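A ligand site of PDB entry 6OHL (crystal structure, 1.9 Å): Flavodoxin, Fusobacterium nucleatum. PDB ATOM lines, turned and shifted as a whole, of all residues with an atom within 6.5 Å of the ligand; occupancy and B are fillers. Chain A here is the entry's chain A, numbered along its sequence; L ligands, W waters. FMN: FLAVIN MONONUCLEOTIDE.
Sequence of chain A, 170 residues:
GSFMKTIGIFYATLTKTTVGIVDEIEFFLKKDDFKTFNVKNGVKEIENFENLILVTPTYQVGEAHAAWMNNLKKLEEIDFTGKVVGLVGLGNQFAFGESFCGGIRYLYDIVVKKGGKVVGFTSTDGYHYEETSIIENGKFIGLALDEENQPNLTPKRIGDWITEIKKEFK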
ATOM      1  N   ALA A  12     -29.170  11.548 -19.569  1.00  0.00           N
ATOM      2  CA  ALA A  12     -30.508  12.014 -19.243  1.00  0.00           C
ATOM      3  C   ALA A  12     -30.701  13.393 -19.893  1.00  0.00           C
ATOM      4  O   ALA A  12     -29.729  14.051 -20.270  1.00  0.00           O
ATOM      5  CB  ALA A  12     -30.714  12.121 -17.733  1.00  0.00           C
ATOM      6  N   THR A  13     -31.965  13.834 -19.998  1.00  0.00           N
ATOM      7  CA  THR A  13     -32.223  15.142 -20.590  1.00  0.00           C
ATOM      8  C   THR A  13     -33.569  15.670 -20.091  1.00  0.00           C
ATOM      9  O   THR A  13     -34.502  14.902 -19.857  1.00  0.00           O
ATOM     10  CB  THR A  13     -32.221  15.082 -22.131  1.00  0.00           C
ATOM     11  OG1 THR A  13     -32.338  16.396 -22.666  1.00  0.00           O
ATOM     12  CG2 THR A  13     -33.348  14.217 -22.658  1.00  0.00           C
ATOM     13  N   LEU A  14     -33.647  16.993 -19.946  1.00  0.00           N
ATOM     14  CA  LEU A  14     -34.940  17.656 -19.746  1.00  0.00           C
ATOM     15  C   LEU A  14     -35.416  18.310 -21.033  1.00  0.00           C
ATOM     16  O   LEU A  14     -36.496  17.980 -21.531  1.00  0.00           O
ATOM     17  CB  LEU A  14     -34.861  18.722 -18.640  1.00  0.00           C
ATOM     18  CG  LEU A  14     -36.187  19.469 -18.394  1.00  0.00           C
ATOM     19  CD1 LEU A  14     -37.284  18.511 -17.891  1.00  0.00           C
ATOM     20  CD2 LEU A  14     -36.006  20.633 -17.419  1.00  0.00           C
ATOM     21  N   THR A  15     -34.619  19.222 -21.606  1.00  0.00           N
ATOM     22  CA  THR A  15     -35.073  19.960 -22.783  1.00  0.00           C
ATOM     23  C   THR A  15     -34.339  19.559 -24.058  1.00  0.00           C
ATOM     24  O   THR A  15     -34.308  20.320 -25.040  1.00  0.00           O
ATOM     25  CB  THR A  15     -34.991  21.471 -22.539  1.00  0.00           C
ATOM     26  OG1 THR A  15     -33.690  21.840 -22.049  1.00  0.00           O
ATOM     27  CG2 THR A  15     -36.030  21.864 -21.513  1.00  0.00           C
ATOM     28  N   LYS A  16     -33.802  18.351 -24.099  1.00  0.00           N
ATOM     29  CA  LYS A  16     -33.330  17.643 -25.283  1.00  0.00           C
ATOM     30  C   LYS A  16     -31.948  18.111 -25.760  1.00  0.00           C
ATOM     31  O   LYS A  16     -31.469  17.548 -26.718  1.00  0.00           O
ATOM     32  CB  LYS A  16     -34.300  17.737 -26.491  1.00  0.00           C
ATOM     33  CG  LYS A  16     -35.767  17.360 -26.192  1.00  0.00           C
ATOM     34  CD  LYS A  16     -35.854  15.926 -25.678  1.00  0.00           C
ATOM     35  CE  LYS A  16     -37.314  15.480 -25.496  1.00  0.00           C
ATOM     36  NZ  LYS A  16     -37.487  14.709 -24.214  1.00  0.00           N
ATOM     37  N   THR A  17     -31.322  19.121 -25.161  1.00  0.00           N
ATOM     38  CA  THR A  17     -29.973  19.517 -25.595  1.00  0.00           C
ATOM     39  C   THR A  17     -29.024  18.315 -25.555  1.00  0.00           C
ATOM     40  O   THR A  17     -28.246  18.081 -26.486  1.00  0.00           O
ATOM     41  CB  THR A  17     -29.415  20.623 -24.708  1.00  0.00           C
ATOM     42  OG1 THR A  17     -30.411  21.664 -24.515  1.00  0.00           O
ATOM     43  CG2 THR A  17     -28.165  21.237 -25.334  1.00  0.00           C
ATOM     44  N   THR A  18     -29.075  17.557 -24.452  1.00  0.00           N
ATOM     45  CA  THR A  18     -28.207  16.383 -24.288  1.00  0.00           C
ATOM     46  C   THR A  18     -28.398  15.355 -25.406  1.00  0.00           C
ATOM     47  O   THR A  18     -27.455  14.663 -25.784  1.00  0.00           O
ATOM     48  CB  THR A  18     -28.461  15.765 -22.905  1.00  0.00           C
ATOM     49  OG1 THR A  18     -28.239  16.768 -21.911  1.00  0.00           O
ATOM     50  CG2 THR A  18     -27.482  14.604 -22.596  1.00  0.00           C
ATOM     51  N   VAL A  19     -29.622  15.241 -25.958  1.00  0.00           N
ATOM     52  CA  VAL A  19     -29.858  14.293 -27.042  1.00  0.00           C
ATOM     53  C   VAL A  19     -28.955  14.590 -28.244  1.00  0.00           C
ATOM     54  O   VAL A  19     -28.415  13.671 -28.886  1.00  0.00           O
ATOM     55  CB  VAL A  19     -31.342  14.327 -27.453  1.00  0.00           C
ATOM     56  CG1 VAL A  19     -31.587  13.451 -28.674  1.00  0.00           C
ATOM     57  CG2 VAL A  19     -32.240  13.907 -26.271  1.00  0.00           C
ATOM     58  N   THR A  56     -24.514  13.972 -18.343  1.00  0.00           N
ATOM     59  CA  THR A  56     -25.662  14.608 -17.728  1.00  0.00           C
ATOM     60  C   THR A  56     -25.638  16.113 -17.915  1.00  0.00           C
ATOM     61  O   THR A  56     -24.580  16.741 -17.741  1.00  0.00           O
ATOM     62  CB  THR A  56     -25.771  14.285 -16.234  1.00  0.00           C
ATOM     63  OG1 THR A  56     -26.931  14.949 -15.703  1.00  0.00           O
ATOM     64  CG2 THR A  56     -24.541  14.741 -15.433  1.00  0.00           C
ATOM     65  N   PRO A  57     -26.773  16.715 -18.225  1.00  0.00           N
ATOM     66  CA  PRO A  57     -26.910  18.165 -18.051  1.00  0.00           C
ATOM     67  C   PRO A  57     -26.976  18.493 -16.561  1.00  0.00           C
ATOM     68  O   PRO A  57     -27.097  17.599 -15.710  1.00  0.00           O
ATOM     69  CB  PRO A  57     -28.226  18.500 -18.760  1.00  0.00           C
ATOM     70  CG  PRO A  57     -29.069  17.258 -18.510  1.00  0.00           C
ATOM     71  CD  PRO A  57     -28.056  16.061 -18.554  1.00  0.00           C
ATOM     72  N   THR A  58     -26.889  19.774 -16.245  1.00  0.00           N
ATOM     73  CA  THR A  58     -26.780  20.221 -14.856  1.00  0.00           C
ATOM     74  C   THR A  58     -28.055  20.932 -14.412  1.00  0.00           C
ATOM     75  O   THR A  58     -28.532  21.827 -15.098  1.00  0.00           O
ATOM     76  CB  THR A  58     -25.609  21.161 -14.656  1.00  0.00           C
ATOM     77  OG1 THR A  58     -24.435  20.595 -15.263  1.00  0.00           O
ATOM     78  CG2 THR A  58     -25.334  21.366 -13.160  1.00  0.00           C
ATOM     79  N   TYR A  59     -28.549  20.570 -13.227  1.00  0.00           N
ATOM     80  CA  TYR A  59     -29.756  21.172 -12.668  1.00  0.00           C
ATOM     81  C   TYR A  59     -29.537  21.422 -11.174  1.00  0.00           C
ATOM     82  O   TYR A  59     -28.592  20.913 -10.578  1.00  0.00           O
ATOM     83  CB  TYR A  59     -30.983  20.270 -12.952  1.00  0.00           C
ATOM     84  CG  TYR A  59     -31.393  20.374 -14.408  1.00  0.00           C
ATOM     85  CD1 TYR A  59     -32.223  21.415 -14.824  1.00  0.00           C
ATOM     86  CD2 TYR A  59     -30.919  19.466 -15.361  1.00  0.00           C
ATOM     87  CE1 TYR A  59     -32.574  21.562 -16.143  1.00  0.00           C
ATOM     88  CE2 TYR A  59     -31.278  19.604 -16.711  1.00  0.00           C
ATOM     89  CZ  TYR A  59     -32.110  20.663 -17.090  1.00  0.00           C
ATOM     90  OH  TYR A  59     -32.475  20.848 -18.400  1.00  0.00           O
ATOM     91  N   GLN A  60     -30.418  22.216 -10.557  1.00  0.00           N
ATOM     92  CA  GLN A  60     -30.538  22.314  -9.080  1.00  0.00           C
ATOM     93  C   GLN A  60     -29.191  22.510  -8.377  1.00  0.00           C
ATOM     94  O   GLN A  60     -28.738  21.671  -7.594  1.00  0.00           O
ATOM     95  CB  GLN A  60     -31.233  21.057  -8.534  1.00  0.00           C
ATOM     96  CG  GLN A  60     -31.960  21.236  -7.210  1.00  0.00           C
ATOM     97  CD  GLN A  60     -33.116  20.267  -7.041  1.00  0.00           C
ATOM     98  OE1 GLN A  60     -34.274  20.647  -7.162  1.00  0.00           O
ATOM     99  NE2 GLN A  60     -32.804  18.991  -6.752  1.00  0.00           N
ATOM    100  N   VAL A  61     -28.548  23.644  -8.639  1.00  0.00           N
ATOM    101  CA  VAL A  61     -27.284  23.993  -7.993  1.00  0.00           C
ATOM    102  C   VAL A  61     -26.247  22.893  -8.172  1.00  0.00           C
ATOM    103  O   VAL A  61     -25.749  22.294  -7.201  1.00  0.00           O
ATOM    104  CB  VAL A  61     -27.468  24.327  -6.496  1.00  0.00           C
ATOM    105  CG1 VAL A  61     -26.202  24.987  -5.983  1.00  0.00           C
ATOM    106  CG2 VAL A  61     -28.640  25.293  -6.308  1.00  0.00           C
ATOM    107  N   GLY A  62     -25.875  22.624  -9.417  1.00  0.00           N
ATOM    108  CA  GLY A  62     -24.746  21.756  -9.639  1.00  0.00           C
ATOM    109  C   GLY A  62     -25.054  20.288  -9.602  1.00  0.00           C
ATOM    110  O   GLY A  62     -24.126  19.475  -9.615  1.00  0.00           O
ATOM    111  N   GLU A  63     -26.325  19.910  -9.526  1.00  0.00           N
ATOM    112  CA  GLU A  63     -26.659  18.500  -9.510  1.00  0.00           C
ATOM    113  C   GLU A  63     -26.755  17.949 -10.933  1.00  0.00           C
ATOM    114  O   GLU A  63     -26.805  18.685 -11.924  1.00  0.00           O
ATOM    115  CB  GLU A  63     -27.994  18.249  -8.796  1.00  0.00           C
ATOM    116  CG  GLU A  63     -27.917  18.526  -7.295  1.00  0.00           C
ATOM    117  CD  GLU A  63     -29.210  18.188  -6.592  1.00  0.00           C
ATOM    118  OE1 GLU A  63     -30.179  17.788  -7.271  1.00  0.00           O
ATOM    119  OE2 GLU A  63     -29.234  18.302  -5.353  1.00  0.00           O
ATOM    120  N   HIS A  65     -29.101  15.679 -13.664  1.00  0.00           N
ATOM    121  CA  HIS A  65     -30.525  15.523 -13.929  1.00  0.00           C
ATOM    122  C   HIS A  65     -31.138  14.596 -12.884  1.00  0.00           C
ATOM    123  O   HIS A  65     -30.493  13.662 -12.396  1.00  0.00           O
ATOM    124  CB  HIS A  65     -30.689  14.964 -15.332  1.00  0.00           C
ATOM    125  CG  HIS A  65     -32.098  14.877 -15.833  1.00  0.00           C
ATOM    126  ND1 HIS A  65     -32.984  13.894 -15.407  1.00  0.00           N
ATOM    127  CD2 HIS A  65     -32.750  15.578 -16.788  1.00  0.00           C
ATOM    128  CE1 HIS A  65     -34.123  14.025 -16.058  1.00  0.00           C
ATOM    129  NE2 HIS A  65     -34.012  15.045 -16.902  1.00  0.00           N
ATOM    130  N   LEU A  90     -23.201  18.944 -19.470  1.00  0.00           N
ATOM    131  CA  LEU A  90     -23.674  20.118 -20.186  1.00  0.00           C
ATOM    132  C   LEU A  90     -24.104  21.128 -19.146  1.00  0.00           C
ATOM    133  O   LEU A  90     -24.722  20.773 -18.135  1.00  0.00           O
ATOM    134  CB  LEU A  90     -24.877  19.808 -21.104  1.00  0.00           C
ATOM    135  CG  LEU A  90     -24.653  19.010 -22.378  1.00  0.00           C
ATOM    136  CD1 LEU A  90     -24.561  17.500 -22.061  1.00  0.00           C
ATOM    137  CD2 LEU A  90     -25.866  19.310 -23.246  1.00  0.00           C
ATOM    138  N   GLY A  91     -23.788  22.401 -19.383  1.00  0.00           N
ATOM    139  CA  GLY A  91     -24.196  23.410 -18.433  1.00  0.00           C
ATOM    140  C   GLY A  91     -24.158  24.766 -19.105  1.00  0.00           C
ATOM    141  O   GLY A  91     -24.058  24.878 -20.324  1.00  0.00           O
ATOM    142  N   ASN A  92     -24.267  25.803 -18.281  1.00  0.00           N
ATOM    143  CA  ASN A  92     -24.171  27.182 -18.757  1.00  0.00           C
ATOM    144  C   ASN A  92     -23.215  27.903 -17.817  1.00  0.00           C
ATOM    145  O   ASN A  92     -23.543  28.167 -16.657  1.00  0.00           O
ATOM    146  CB  ASN A  92     -25.551  27.868 -18.791  1.00  0.00           C
ATOM    147  CG  ASN A  92     -25.474  29.332 -19.220  1.00  0.00           C
ATOM    148  OD1 ASN A  92     -24.481  30.009 -18.956  1.00  0.00           O
ATOM    149  ND2 ASN A  92     -26.521  29.830 -19.854  1.00  0.00           N
ATOM    150  N   GLN A  93     -22.012  28.243 -18.328  1.00  0.00           N
ATOM    151  CA  GLN A  93     -20.959  28.700 -17.416  1.00  0.00           C
ATOM    152  C   GLN A  93     -21.139  30.126 -16.918  1.00  0.00           C
ATOM    153  O   GLN A  93     -20.552  30.471 -15.891  1.00  0.00           O
ATOM    154  CB  GLN A  93     -19.574  28.577 -18.086  1.00  0.00           C
ATOM    155  CG  GLN A  93     -19.361  29.519 -19.267  1.00  0.00           C
ATOM    156  CD  GLN A  93     -18.288  29.002 -20.223  1.00  0.00           C
ATOM    157  OE1 GLN A  93     -17.092  29.284 -20.036  1.00  0.00           O
ATOM    158  NE2 GLN A  93     -18.702  28.234 -21.211  1.00  0.00           N
ATOM    159  N   PHE A  96     -24.406  30.130 -14.384  1.00  0.00           N
ATOM    160  CA  PHE A  96     -24.155  29.355 -13.173  1.00  0.00           C
ATOM    161  C   PHE A  96     -22.660  29.390 -12.884  1.00  0.00           C
ATOM    162  O   PHE A  96     -21.960  28.384 -13.071  1.00  0.00           O
ATOM    163  CB  PHE A  96     -24.689  27.939 -13.301  1.00  0.00           C
ATOM    164  CG  PHE A  96     -26.171  27.908 -13.579  1.00  0.00           C
ATOM    165  CD1 PHE A  96     -27.092  27.986 -12.531  1.00  0.00           C
ATOM    166  CD2 PHE A  96     -26.643  27.909 -14.884  1.00  0.00           C
ATOM    167  CE1 PHE A  96     -28.464  28.009 -12.780  1.00  0.00           C
ATOM    168  CE2 PHE A  96     -28.011  27.927 -15.152  1.00  0.00           C
ATOM    169  CZ  PHE A  96     -28.932  27.994 -14.090  1.00  0.00           C
ATOM    170  N   SER A  99     -21.495  26.577 -10.392  1.00  0.00           N
ATOM    171  CA  SER A  99     -21.983  25.206 -10.479  1.00  0.00           C
ATOM    172  C   SER A  99     -21.988  24.706 -11.929  1.00  0.00           C
ATOM    173  O   SER A  99     -22.788  23.837 -12.284  1.00  0.00           O
ATOM    174  CB  SER A  99     -23.388  25.091  -9.889  1.00  0.00           C
ATOM    175  OG  SER A  99     -24.215  26.061 -10.485  1.00  0.00           O
ATOM    176  N   PHE A 100     -21.092  25.241 -12.752  1.00  0.00           N
ATOM    177  CA  PHE A 100     -21.032  24.861 -14.167  1.00  0.00           C
ATOM    178  C   PHE A 100     -20.673  23.386 -14.312  1.00  0.00           C
ATOM    179  O   PHE A 100     -19.616  22.944 -13.827  1.00  0.00           O
ATOM    180  CB  PHE A 100     -20.011  25.716 -14.912  1.00  0.00           C
ATOM    181  CG  PHE A 100     -19.790  25.317 -16.364  1.00  0.00           C
ATOM    182  CD1 PHE A 100     -20.842  25.274 -17.269  1.00  0.00           C
ATOM    183  CD2 PHE A 100     -18.521  24.973 -16.810  1.00  0.00           C
ATOM    184  CE1 PHE A 100     -20.646  24.919 -18.610  1.00  0.00           C
ATOM    185  CE2 PHE A 100     -18.303  24.613 -18.146  1.00  0.00           C
ATOM    186  CZ  PHE A 100     -19.366  24.593 -19.048  1.00  0.00           C
ATOM    187  N   CYS A 101     -21.553  22.631 -14.975  1.00  0.00           N
ATOM    188  CA  CYS A 101     -21.377  21.184 -15.174  1.00  0.00           C
ATOM    189  C   CYS A 101     -21.134  20.451 -13.860  1.00  0.00           C
ATOM    190  O   CYS A 101     -20.438  19.430 -13.834  1.00  0.00           O
ATOM    191  CB  CYS A 101     -20.232  20.904 -16.145  1.00  0.00           C
ATOM    192  SG  CYS A 101     -20.701  21.251 -17.876  1.00  0.00           S
ATOM    193  N   GLY A 102     -21.719  20.932 -12.766  1.00  0.00           N
ATOM    194  CA  GLY A 102     -21.457  20.298 -11.475  1.00  0.00           C
ATOM    195  C   GLY A 102     -21.988  18.890 -11.362  1.00  0.00           C
ATOM    196  O   GLY A 102     -21.572  18.143 -10.473  1.00  0.00           O
ATOM    197  N   LEU A 145     -19.430  20.931 -21.549  1.00  0.00           N
ATOM    198  CA  LEU A 145     -20.011  21.538 -22.729  1.00  0.00           C
ATOM    199  C   LEU A 145     -20.963  22.654 -22.336  1.00  0.00           C
ATOM    200  O   LEU A 145     -21.667  22.563 -21.327  1.00  0.00           O
ATOM    201  CB  LEU A 145     -20.736  20.483 -23.567  1.00  0.00           C
ATOM    202  CG  LEU A 145     -19.802  19.331 -23.954  1.00  0.00           C
ATOM    203  CD1 LEU A 145     -20.597  18.242 -24.650  1.00  0.00           C
ATOM    204  CD2 LEU A 145     -18.678  19.842 -24.830  1.00  0.00           C
ATOM    205  N   GLU A 147     -23.735  24.654 -24.464  1.00  0.00           N
ATOM    206  CA  GLU A 147     -24.445  24.867 -25.724  1.00  0.00           C
ATOM    207  C   GLU A 147     -25.055  26.264 -25.832  1.00  0.00           C
ATOM    208  O   GLU A 147     -25.405  26.688 -26.949  1.00  0.00           O
ATOM    209  CB  GLU A 147     -25.566  23.837 -25.891  1.00  0.00           C
ATOM    210  CG  GLU A 147     -25.131  22.555 -26.481  1.00  0.00           C
ATOM    211  CD  GLU A 147     -24.432  22.722 -27.826  1.00  0.00           C
ATOM    212  OE1 GLU A 147     -25.083  22.842 -28.882  1.00  0.00           O
ATOM    213  OE2 GLU A 147     -23.207  22.719 -27.801  1.00  0.00           O
ATOM    214  N   GLU A 148     -25.268  26.948 -24.705  1.00  0.00           N
ATOM    215  CA  GLU A 148     -25.795  28.307 -24.764  1.00  0.00           C
ATOM    216  C   GLU A 148     -24.715  29.284 -25.224  1.00  0.00           C
ATOM    217  O   GLU A 148     -24.928  30.069 -26.145  1.00  0.00           O
ATOM    218  CB  GLU A 148     -26.323  28.742 -23.405  1.00  0.00           C
ATOM    219  CG  GLU A 148     -27.646  28.124 -23.035  1.00  0.00           C
ATOM    220  CD  GLU A 148     -27.520  26.976 -22.037  1.00  0.00           C
ATOM    221  OE1 GLU A 148     -26.457  26.306 -21.976  1.00  0.00           O
ATOM    222  OE2 GLU A 148     -28.493  26.743 -21.297  1.00  0.00           O
HETATM  223  N1  FMN L   1     -26.151  24.649 -15.873  1.00  0.00           N
HETATM  224  C2  FMN L   1     -25.068  24.556 -15.043  1.00  0.00           C
HETATM  225  O2  FMN L   1     -23.909  24.537 -15.480  1.00  0.00           O
HETATM  226  N3  FMN L   1     -25.222  24.515 -13.684  1.00  0.00           N
HETATM  227  C4  FMN L   1     -26.467  24.527 -13.115  1.00  0.00           C
HETATM  228  O4  FMN L   1     -26.536  24.467 -11.903  1.00  0.00           O
HETATM  229  C4A FMN L   1     -27.588  24.627 -13.934  1.00  0.00           C
HETATM  230  N5  FMN L   1     -28.838  24.653 -13.391  1.00  0.00           N
HETATM  231  C5A FMN L   1     -29.931  24.744 -14.202  1.00  0.00           C
HETATM  232  C6  FMN L   1     -31.189  24.784 -13.579  1.00  0.00           C
HETATM  233  C7  FMN L   1     -32.319  24.868 -14.375  1.00  0.00           C
HETATM  234  C7M FMN L   1     -33.682  24.894 -13.717  1.00  0.00           C
HETATM  235  C8  FMN L   1     -32.194  24.930 -15.755  1.00  0.00           C
HETATM  236  C8M FMN L   1     -33.420  25.048 -16.610  1.00  0.00           C
HETATM  237  C9  FMN L   1     -30.939  24.906 -16.372  1.00  0.00           C
HETATM  238  C9A FMN L   1     -29.792  24.808 -15.580  1.00  0.00           C
HETATM  239  N10 FMN L   1     -28.518  24.747 -16.151  1.00  0.00           N
HETATM  240  C10 FMN L   1     -27.419  24.692 -15.317  1.00  0.00           C
HETATM  241  C1' FMN L   1     -28.298  24.801 -17.616  1.00  0.00           C
HETATM  242  C2' FMN L   1     -28.538  23.405 -18.268  1.00  0.00           C
HETATM  243  O2' FMN L   1     -27.772  22.371 -17.646  1.00  0.00           O
HETATM  244  C3' FMN L   1     -28.236  23.479 -19.764  1.00  0.00           C
HETATM  245  O3' FMN L   1     -29.180  24.394 -20.307  1.00  0.00           O
HETATM  246  C4' FMN L   1     -28.323  22.143 -20.517  1.00  0.00           C
HETATM  247  O4' FMN L   1     -27.986  22.292 -21.889  1.00  0.00           O
HETATM  248  C5' FMN L   1     -29.712  21.525 -20.445  1.00  0.00           C
HETATM  249  O5' FMN L   1     -29.673  20.275 -21.111  1.00  0.00           O
HETATM  250  P   FMN L   1     -30.993  19.422 -21.532  1.00  0.00           P
HETATM  251  O1P FMN L   1     -31.843  19.283 -20.256  1.00  0.00           O
HETATM  252  O2P FMN L   1     -30.554  18.100 -22.110  1.00  0.00           O
HETATM  253  O3P FMN L   1     -31.773  20.208 -22.567  1.00  0.00           O
HETATM  254  O   HOH W   1     -29.454  24.068 -23.592  1.00  0.00           O
HETATM  255  O   HOH W   2     -29.236  25.545 -10.482  1.00  0.00           O
HETATM  256  O   HOH W   3     -25.556  23.673 -22.141  1.00  0.00           O
HETATM  257  O   HOH W   4     -31.849  25.306 -19.942  1.00  0.00           O
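OG1 of Thr 15 is in hydrogen-bond range of O3P of the ligand, at 2.6 Å.
The backbone NH (N) of Lys 16 sits at hydrogen-bond distance from an oxygen (O3P) of the ligand, 3.1 Å away.
The side-chain hydroxyl of Ser 99 is in hydrogen-bond range of an oxygen (O4) of the ligand (3.2 Å).
The backbone NH (N) of Thr 15 lies within hydrogen-bond range of an oxygen (O1P) of the ligand (3.1 Å).
The backbone NH of Thr 18 sits at hydrogen-bond distance from an oxygen (O2P) of the ligand (2.8 Å).
O2' of the ligand lies within hydrogen-bond range of O of Leu 90 (3.5 Å).
O2P of the ligand sits at hydrogen-bond distance from OG1 of Thr 18, at 2.7 Å.
An oxygen (O2) of the ligand lies within hydrogen-bond range of the backbone NH (N) of Asn 92 (3.1 Å).
O1P of the ligand lies within hydrogen-bond range of OH of Tyr 59.
OE2 of Glu 148 lies within hydrogen-bond range of O3' of the ligand (2.6 Å).
The side-chain hydroxyl (OG1) of Thr 17 lies within hydrogen-bond range of an oxygen (O3P) of the ligand (2.8 Å).
An oxygen (O2P) of the ligand is in hydrogen-bond range of the side-chain hydroxyl (OG1) of Thr 13, 2.5 Å away.
The backbone NH (N) of Leu 14 is in hydrogen-bond range of an oxygen (O1P) of the ligand.
O of Thr 58 sits at hydrogen-bond distance from O2' of the ligand (2.7 Å).
O of Ser 99 lies within hydrogen-bond range of N3 of the ligand, at 2.9 Å.
O3P of the ligand sits at hydrogen-bond distance from N of Thr 17, 2.8 Å away.
The backbone NH (N) of Gly 62 is in hydrogen-bond range of an oxygen (O4) of the ligand.
The backbone NH (N) of Cys 101 sits at hydrogen-bond distance from an oxygen (O2) of the ligand (3.1 Å).
N of Thr 58 sits at hydrogen-bond distance from O2' of the ligand (3.1 Å).
The side-chain sulfur (SG) of Cys 101 sits close to the backbone NH (N) of Leu 90, at 3.8 Å.
The side-chain hydroxyl (OG1) of Thr 13 lies within hydrogen-bond range of the backbone NH (N) of Lys 16, at 2.8 Å.
The backbone NH of Gly 91 is in hydrogen-bond range of the backbone carbonyl oxygen of Leu 145.
The side-chain sulfur of Cys 101 is in hydrogen-bond range of the backbone NH of Gly 91, at 3.6 Å.
N of His 65 lies within hydrogen-bond range of O of Pro 57.
A ring nitrogen (NE2) of His 65 is in hydrogen-bond range of the backbone carbonyl oxygen of Thr 13 (3.0 Å).
N of Leu 90 sits at hydrogen-bond distance from O of Thr 56.
The side-chain hydroxyl (OG1) of Thr 58 lies within hydrogen-bond range of the backbone carbonyl oxygen (O) of Leu 90.
CB of Pro 57 touches O5' of the ligand, 3.3 Å away.
N of Val 61 touches O4 of the ligand (3.9 Å).
CA of Gly 91 touches O2 of the ligand, at 3.2 Å.
Phe 96 touches the ligand.
Phe 100 touches the ligand (CA to O2, 3.2 Å).
Hydrophobic or aromatic side chains within 4 Å of the ligand: Leu 14, Pro 57, Tyr 59, Leu 90, Phe 96 and Phe 100.
Water W3 lies within hydrogen-bond range of the backbone carbonyl oxygen of Gly 91 (2.6 Å), the side-chain carboxylate of Glu 148 (2.8 Å), an oxygen (O4') of the ligand (2.8 Å) and the backbone NH of Glu 147 (3.1 Å).
Water W1 lies within hydrogen-bond range of OG1 of Thr 17 and O4' of the ligand.
Water W2 bridges N of Val 61 (2.7 Å) and N5 of the ligand (3.1 Å).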
